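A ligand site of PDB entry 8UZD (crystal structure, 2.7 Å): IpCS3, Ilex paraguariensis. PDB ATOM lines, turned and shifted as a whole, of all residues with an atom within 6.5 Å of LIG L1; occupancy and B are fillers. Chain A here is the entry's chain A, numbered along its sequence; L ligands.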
ATOM      1  N   PHE A  26       2.762 -13.089  11.811  1.00  0.00           N
ATOM      2  CA  PHE A  26       2.279 -12.286  12.936  1.00  0.00           C
ATOM      3  C   PHE A  26       1.345 -11.162  12.482  1.00  0.00           C
ATOM      4  O   PHE A  26       0.191 -11.098  12.925  1.00  0.00           O
ATOM      5  CB  PHE A  26       3.424 -11.780  13.824  1.00  0.00           C
ATOM      6  CG  PHE A  26       2.947 -11.020  15.045  1.00  0.00           C
ATOM      7  CD1 PHE A  26       2.554 -11.689  16.193  1.00  0.00           C
ATOM      8  CD2 PHE A  26       2.856  -9.630  15.024  1.00  0.00           C
ATOM      9  CE1 PHE A  26       2.106 -10.992  17.308  1.00  0.00           C
ATOM     10  CE2 PHE A  26       2.386  -8.932  16.126  1.00  0.00           C
ATOM     11  CZ  PHE A  26       2.011  -9.613  17.268  1.00  0.00           C
ATOM     12  N   SER A  27       1.853 -10.259  11.633  1.00  0.00           N
ATOM     13  CA  SER A  27       1.046  -9.181  11.099  1.00  0.00           C
ATOM     14  C   SER A  27      -0.251  -9.715  10.498  1.00  0.00           C
ATOM     15  O   SER A  27      -1.314  -9.092  10.644  1.00  0.00           O
ATOM     16  CB  SER A  27       1.819  -8.364  10.095  1.00  0.00           C
ATOM     17  OG  SER A  27       1.020  -7.310   9.594  1.00  0.00           O
ATOM     18  N   TYR A 154      -1.729  -0.998  15.145  1.00  0.00           N
ATOM     19  CA  TYR A 154      -0.301  -0.975  15.434  1.00  0.00           C
ATOM     20  C   TYR A 154       0.345   0.391  15.200  1.00  0.00           C
ATOM     21  O   TYR A 154       1.474   0.461  14.680  1.00  0.00           O
ATOM     22  CB  TYR A 154       0.381  -2.200  14.808  1.00  0.00           C
ATOM     23  CG  TYR A 154       0.521  -3.333  15.783  1.00  0.00           C
ATOM     24  CD1 TYR A 154      -0.610  -3.958  16.314  1.00  0.00           C
ATOM     25  CD2 TYR A 154       1.765  -3.775  16.206  1.00  0.00           C
ATOM     26  CE1 TYR A 154      -0.498  -4.997  17.231  1.00  0.00           C
ATOM     27  CE2 TYR A 154       1.897  -4.802  17.123  1.00  0.00           C
ATOM     28  CZ  TYR A 154       0.759  -5.407  17.643  1.00  0.00           C
ATOM     29  OH  TYR A 154       0.871  -6.400  18.564  1.00  0.00           O
ATOM     30  N   SER A 155      -0.323   1.474  15.637  1.00  0.00           N
ATOM     31  CA  SER A 155       0.244   2.819  15.492  1.00  0.00           C
ATOM     32  C   SER A 155       0.265   3.555  16.825  1.00  0.00           C
ATOM     33  O   SER A 155       1.250   4.188  17.172  1.00  0.00           O
ATOM     34  CB  SER A 155      -0.514   3.636  14.487  1.00  0.00           C
ATOM     35  OG  SER A 155      -0.717   2.920  13.289  1.00  0.00           O
ATOM     36  N   HIS A 157       0.580   3.087  19.747  1.00  0.00           N
ATOM     37  CA  HIS A 157       1.458   2.784  20.868  1.00  0.00           C
ATOM     38  C   HIS A 157       2.710   3.649  20.803  1.00  0.00           C
ATOM     39  O   HIS A 157       3.443   3.731  21.777  1.00  0.00           O
ATOM     40  CB  HIS A 157       1.769   1.277  20.954  1.00  0.00           C
ATOM     41  CG  HIS A 157       2.267   0.698  19.671  1.00  0.00           C
ATOM     42  ND1 HIS A 157       1.630  -0.350  19.032  1.00  0.00           N
ATOM     43  CD2 HIS A 157       3.316   1.020  18.890  1.00  0.00           C
ATOM     44  CE1 HIS A 157       2.271  -0.665  17.928  1.00  0.00           C
ATOM     45  NE2 HIS A 157       3.301   0.164  17.811  1.00  0.00           N
ATOM     46  N   TRP A 158       2.940   4.287  19.640  1.00  0.00           N
ATOM     47  CA  TRP A 158       4.057   5.197  19.444  1.00  0.00           C
ATOM     48  C   TRP A 158       3.723   6.543  20.088  1.00  0.00           C
ATOM     49  O   TRP A 158       2.649   7.080  19.845  1.00  0.00           O
ATOM     50  CB  TRP A 158       4.337   5.395  17.953  1.00  0.00           C
ATOM     51  CG  TRP A 158       4.831   4.192  17.238  1.00  0.00           C
ATOM     52  CD1 TRP A 158       4.161   3.423  16.332  1.00  0.00           C
ATOM     53  CD2 TRP A 158       6.145   3.622  17.340  1.00  0.00           C
ATOM     54  NE1 TRP A 158       4.957   2.414  15.874  1.00  0.00           N
ATOM     55  CE2 TRP A 158       6.187   2.507  16.479  1.00  0.00           C
ATOM     56  CE3 TRP A 158       7.289   3.949  18.087  1.00  0.00           C
ATOM     57  CZ2 TRP A 158       7.333   1.735  16.337  1.00  0.00           C
ATOM     58  CZ3 TRP A 158       8.413   3.163  17.959  1.00  0.00           C
ATOM     59  CH2 TRP A 158       8.434   2.084  17.080  1.00  0.00           C
ATOM     60  N   ASN A 223       0.032  -2.676  20.158  1.00  0.00           N
ATOM     61  CA  ASN A 223       0.927  -3.545  20.897  1.00  0.00           C
ATOM     62  C   ASN A 223       0.776  -3.212  22.383  1.00  0.00           C
ATOM     63  O   ASN A 223       0.743  -2.041  22.732  1.00  0.00           O
ATOM     64  CB  ASN A 223       2.354  -3.422  20.353  1.00  0.00           C
ATOM     65  CG  ASN A 223       3.346  -4.293  21.076  1.00  0.00           C
ATOM     66  OD1 ASN A 223       4.315  -3.787  21.634  1.00  0.00           O
ATOM     67  ND2 ASN A 223       3.125  -5.602  21.084  1.00  0.00           N
ATOM     68  N   SER A 235       6.758  -8.841  27.436  1.00  0.00           N
ATOM     69  CA  SER A 235       5.919  -7.819  26.836  1.00  0.00           C
ATOM     70  C   SER A 235       6.678  -7.015  25.774  1.00  0.00           C
ATOM     71  O   SER A 235       6.099  -6.638  24.760  1.00  0.00           O
ATOM     72  CB  SER A 235       5.310  -6.928  27.888  1.00  0.00           C
ATOM     73  OG  SER A 235       6.055  -6.972  29.103  1.00  0.00           O
ATOM     74  N   HIS A 238      11.255  -7.025  21.714  1.00  0.00           N
ATOM     75  CA  HIS A 238      12.070  -6.347  20.722  1.00  0.00           C
ATOM     76  C   HIS A 238      12.966  -5.295  21.376  1.00  0.00           C
ATOM     77  O   HIS A 238      14.088  -5.080  20.950  1.00  0.00           O
ATOM     78  CB  HIS A 238      11.167  -5.760  19.614  1.00  0.00           C
ATOM     79  CG  HIS A 238       9.877  -5.303  20.175  1.00  0.00           C
ATOM     80  ND1 HIS A 238       8.849  -6.185  20.458  1.00  0.00           N
ATOM     81  CD2 HIS A 238       9.466  -4.085  20.584  1.00  0.00           C
ATOM     82  CE1 HIS A 238       7.853  -5.529  21.007  1.00  0.00           C
ATOM     83  NE2 HIS A 238       8.208  -4.236  21.092  1.00  0.00           N
ATOM     84  N   TRP A 239      12.441  -4.620  22.408  1.00  0.00           N
ATOM     85  CA  TRP A 239      13.202  -3.575  23.075  1.00  0.00           C
ATOM     86  C   TRP A 239      14.311  -4.190  23.925  1.00  0.00           C
ATOM     87  O   TRP A 239      15.358  -3.573  24.118  1.00  0.00           O
ATOM     88  CB  TRP A 239      12.299  -2.635  23.894  1.00  0.00           C
ATOM     89  CG  TRP A 239      11.180  -1.970  23.143  1.00  0.00           C
ATOM     90  CD1 TRP A 239       9.889  -1.808  23.572  1.00  0.00           C
ATOM     91  CD2 TRP A 239      11.243  -1.351  21.842  1.00  0.00           C
ATOM     92  NE1 TRP A 239       9.148  -1.140  22.639  1.00  0.00           N
ATOM     93  CE2 TRP A 239       9.952  -0.849  21.557  1.00  0.00           C
ATOM     94  CE3 TRP A 239      12.250  -1.170  20.890  1.00  0.00           C
ATOM     95  CZ2 TRP A 239       9.650  -0.194  20.368  1.00  0.00           C
ATOM     96  CZ3 TRP A 239      11.947  -0.504  19.711  1.00  0.00           C
ATOM     97  CH2 TRP A 239      10.665  -0.035  19.450  1.00  0.00           C
ATOM     98  N   CYS A 267       7.924   4.674  22.887  1.00  0.00           N
ATOM     99  CA  CYS A 267       6.940   3.627  22.640  1.00  0.00           C
ATOM    100  C   CYS A 267       6.505   3.006  23.962  1.00  0.00           C
ATOM    101  O   CYS A 267       7.349   2.727  24.813  1.00  0.00           O
ATOM    102  CB  CYS A 267       7.582   2.558  21.783  1.00  0.00           C
ATOM    103  SG  CYS A 267       6.357   1.520  20.932  1.00  0.00           S
ATOM    104  N   TYR A 268       5.203   2.746  24.113  1.00  0.00           N
ATOM    105  CA  TYR A 268       4.658   2.114  25.310  1.00  0.00           C
ATOM    106  C   TYR A 268       3.744   0.958  24.955  1.00  0.00           C
ATOM    107  O   TYR A 268       3.033   0.994  23.962  1.00  0.00           O
ATOM    108  CB  TYR A 268       3.867   3.138  26.138  1.00  0.00           C
ATOM    109  CG  TYR A 268       3.407   2.671  27.493  1.00  0.00           C
ATOM    110  CD1 TYR A 268       4.313   2.220  28.442  1.00  0.00           C
ATOM    111  CD2 TYR A 268       2.072   2.725  27.848  1.00  0.00           C
ATOM    112  CE1 TYR A 268       3.903   1.826  29.713  1.00  0.00           C
ATOM    113  CE2 TYR A 268       1.640   2.332  29.107  1.00  0.00           C
ATOM    114  CZ  TYR A 268       2.562   1.891  30.047  1.00  0.00           C
ATOM    115  OH  TYR A 268       2.138   1.492  31.293  1.00  0.00           O
ATOM    116  N   PHE A 297       5.604 -14.778  18.553  1.00  0.00           N
ATOM    117  CA  PHE A 297       6.110 -13.695  17.733  1.00  0.00           C
ATOM    118  C   PHE A 297       6.553 -14.226  16.368  1.00  0.00           C
ATOM    119  O   PHE A 297       6.316 -13.601  15.343  1.00  0.00           O
ATOM    120  CB  PHE A 297       7.278 -12.992  18.429  1.00  0.00           C
ATOM    121  CG  PHE A 297       7.364 -11.503  18.211  1.00  0.00           C
ATOM    122  CD1 PHE A 297       6.904 -10.925  17.036  1.00  0.00           C
ATOM    123  CD2 PHE A 297       7.897 -10.680  19.189  1.00  0.00           C
ATOM    124  CE1 PHE A 297       6.986  -9.555  16.840  1.00  0.00           C
ATOM    125  CE2 PHE A 297       7.979  -9.311  18.993  1.00  0.00           C
ATOM    126  CZ  PHE A 297       7.529  -8.750  17.816  1.00  0.00           C
ATOM    127  N   ASN A 315      11.650  -8.855  10.657  1.00  0.00           N
ATOM    128  CA  ASN A 315      10.402  -8.230  11.068  1.00  0.00           C
ATOM    129  C   ASN A 315      10.694  -7.093  12.039  1.00  0.00           C
ATOM    130  O   ASN A 315      10.187  -5.983  11.856  1.00  0.00           O
ATOM    131  CB  ASN A 315       9.435  -9.256  11.672  1.00  0.00           C
ATOM    132  CG  ASN A 315       8.001  -8.750  11.743  1.00  0.00           C
ATOM    133  OD1 ASN A 315       7.531  -8.311  12.797  1.00  0.00           O
ATOM    134  ND2 ASN A 315       7.300  -8.809  10.625  1.00  0.00           N
ATOM    135  N   SER A 318      12.382  -4.108  10.545  1.00  0.00           N
ATOM    136  CA  SER A 318      11.545  -3.357   9.625  1.00  0.00           C
ATOM    137  C   SER A 318      10.715  -2.295  10.341  1.00  0.00           C
ATOM    138  O   SER A 318      10.265  -1.339   9.701  1.00  0.00           O
ATOM    139  CB  SER A 318      10.677  -4.256   8.784  1.00  0.00           C
ATOM    140  OG  SER A 318       9.396  -4.418   9.374  1.00  0.00           O
ATOM    141  N   PHE A 319      10.494  -2.450  11.648  1.00  0.00           N
ATOM    142  CA  PHE A 319       9.681  -1.481  12.359  1.00  0.00           C
ATOM    143  C   PHE A 319      10.507  -0.723  13.402  1.00  0.00           C
ATOM    144  O   PHE A 319       9.946   0.124  14.096  1.00  0.00           O
ATOM    145  CB  PHE A 319       8.380  -2.096  12.885  1.00  0.00           C
ATOM    146  CG  PHE A 319       8.501  -3.003  14.083  1.00  0.00           C
ATOM    147  CD1 PHE A 319       8.662  -2.494  15.370  1.00  0.00           C
ATOM    148  CD2 PHE A 319       8.433  -4.382  13.944  1.00  0.00           C
ATOM    149  CE1 PHE A 319       8.759  -3.334  16.467  1.00  0.00           C
ATOM    150  CE2 PHE A 319       8.534  -5.230  15.040  1.00  0.00           C
ATOM    151  CZ  PHE A 319       8.702  -4.704  16.310  1.00  0.00           C
ATOM    152  N   ASN A 355       4.163 -12.037  21.782  1.00  0.00           N
ATOM    153  CA  ASN A 355       3.852 -10.625  21.620  1.00  0.00           C
ATOM    154  C   ASN A 355       2.363 -10.407  21.914  1.00  0.00           C
ATOM    155  O   ASN A 355       1.530 -11.240  21.544  1.00  0.00           O
ATOM    156  CB  ASN A 355       4.236 -10.116  20.229  1.00  0.00           C
ATOM    157  CG  ASN A 355       4.409  -8.611  20.192  1.00  0.00           C
ATOM    158  OD1 ASN A 355       4.795  -8.000  21.189  1.00  0.00           O
ATOM    159  ND2 ASN A 355       4.143  -8.010  19.050  1.00  0.00           N
ATOM    160  N   THR A 356       2.026  -9.267  22.536  1.00  0.00           N
ATOM    161  CA  THR A 356       0.692  -9.071  23.061  1.00  0.00           C
ATOM    162  C   THR A 356       0.018  -7.841  22.445  1.00  0.00           C
ATOM    163  O   THR A 356       0.638  -6.804  22.243  1.00  0.00           O
ATOM    164  CB  THR A 356       0.697  -9.035  24.584  1.00  0.00           C
ATOM    165  OG1 THR A 356       1.198 -10.302  24.988  1.00  0.00           O
ATOM    166  CG2 THR A 356      -0.683  -8.863  25.181  1.00  0.00           C
HETATM  167  N1  LIG L   1       5.155  -2.355  15.028  1.00  0.00           N
HETATM  168  C1  LIG L   1       4.997  -3.693  14.611  1.00  0.00           C
HETATM  169  C2  LIG L   1       5.031  -1.299  14.001  1.00  0.00           C
HETATM  170  C3  LIG L   1       5.415  -1.911  16.343  1.00  0.00           C
HETATM  171  N2  LIG L   1       5.091  -4.678  15.574  1.00  0.00           N
HETATM  172  O1  LIG L   1       4.784  -3.968  13.437  1.00  0.00           O
HETATM  173  C4  LIG L   1       4.924  -6.082  15.184  1.00  0.00           C
HETATM  174  C5  LIG L   1       5.333  -4.323  16.879  1.00  0.00           C
HETATM  175  C6  LIG L   1       5.495  -3.002  17.262  1.00  0.00           C
HETATM  176  N3  LIG L   1       5.453  -5.168  17.942  1.00  0.00           N
HETATM  177  O2  LIG L   1       5.532  -0.726  16.601  1.00  0.00           O
HETATM  178  N4  LIG L   1       5.731  -3.027  18.643  1.00  0.00           N
HETATM  179  C7  LIG L   1       5.671  -4.356  18.981  1.00  0.00           C
HETATM  180  C8  LIG L   1       5.956  -1.868  19.508  1.00  0.00           C
HETATM  181  N1  LG2 L   2      -1.421   0.325  10.405  1.00  0.00           N
HETATM  182  C1  LG2 L   2      -0.435  -0.326   9.475  1.00  0.00           C
HETATM  183  C2  LG2 L   2       0.990   0.185   9.719  1.00  0.00           C
HETATM  184  C3  LG2 L   2       1.399   0.212  11.174  1.00  0.00           C
HETATM  185  S1  LG2 L   2       3.055   0.898  11.408  1.00  0.00           S
HETATM  186  C4  LG2 L   2      -0.477  -1.851   9.619  1.00  0.00           C
HETATM  187  O1  LG2 L   2       0.344  -2.517   9.013  1.00  0.00           O
HETATM  188  O2  LG2 L   2      -1.294  -2.491  10.299  1.00  0.00           O
HETATM  189  C5  LG2 L   2       2.729   2.362  12.448  1.00  0.00           C
HETATM  190  C6  LG2 L   2       2.650   3.658  11.654  1.00  0.00           C
HETATM  191  O3  LG2 L   2       2.199   4.743  12.491  1.00  0.00           O
HETATM  192  C7  LG2 L   2       3.975   4.125  11.038  1.00  0.00           C
HETATM  193  O4  LG2 L   2       3.876   4.150   9.620  1.00  0.00           O
HETATM  194  C8  LG2 L   2       4.208   5.517  11.634  1.00  0.00           C
HETATM  195  O5  LG2 L   2       4.786   6.431  10.736  1.00  0.00           O
HETATM  196  C9  LG2 L   2       2.793   5.927  12.006  1.00  0.00           C
HETATM  197  N2  LG2 L   2       2.702   6.960  13.031  1.00  0.00           N
HETATM  198  C10 LG2 L   2       3.374   7.003  14.235  1.00  0.00           C
HETATM  199  N3  LG2 L   2       3.056   8.039  14.955  1.00  0.00           N
HETATM  200  C11 LG2 L   2       2.114   8.735  14.200  1.00  0.00           C
HETATM  201  C12 LG2 L   2       1.382   9.923  14.426  1.00  0.00           C
HETATM  202  N4  LG2 L   2       1.491  10.667  15.520  1.00  0.00           N
HETATM  203  N5  LG2 L   2       0.510  10.313  13.469  1.00  0.00           N
HETATM  204  C13 LG2 L   2       0.405   9.572  12.361  1.00  0.00           C
HETATM  205  N6  LG2 L   2       1.038   8.445  12.039  1.00  0.00           N
HETATM  206  C14 LG2 L   2       1.891   8.064  13.016  1.00  0.00           C
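A nitrogen (N4) of LIG L1 sits close to the side-chain amide oxygen (OD1) of Asn 223, at 3.4 Å. CE2 of Phe 26 touches C4 of LIG L1, at 3.9 Å. Tyr 154 touches LIG L1. His 238 touches LIG L1 (CE1 to C7, 3.2 Å). SG of Cys 267 touches C8 of LIG L1 (3.7 Å). Phe 319 touches LIG L1 (CE1 to C6, 3.4 Å). Hydrophobic or aromatic side chains within 4 Å of LIG L1: Phe 26, Tyr 154, His 157, Trp 158, His 238 and Phe 319. Of the 18 residues printed, 9 come within 4 Å of LIG L1.
O2 of LIG L1 lies within hydrogen-bond range of NE2 of His 157 (2.7 Å). The indole nitrogen of Trp 158 lies close to an oxygen (O2) of LIG L1 (3.3 Å). ND2 of Asn 355 is in hydrogen-bond range of N3 of LIG L1 (3.3 Å).
The backbone NH (N) of Asn 223 lies within hydrogen-bond range of a ring nitrogen (ND1) of His 157, at 3.0 Å. A ring nitrogen (NE2) of His 157 lies within hydrogen-bond range of the indole nitrogen (NE1) of Trp 158 (3.4 Å). ND2 of Asn 223 lies within hydrogen-bond range of O of Thr 356 (3.0 Å). OH of Tyr 154 lies within hydrogen-bond range of ND2 of Asn 223, at 3.5 Å. The backbone carbonyl oxygen (O) of His 157 sits close to the side-chain sulfur (SG) of Cys 267 (3.8 Å). The backbone carbonyl oxygen (O) of His 157 lies within hydrogen-bond range of the backbone NH (N) of Tyr 268 (3.1 Å). The side-chain amide oxygen of Asn 355 lies within hydrogen-bond range of the side-chain amide nitrogen of Asn 223, at 2.9 Å.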
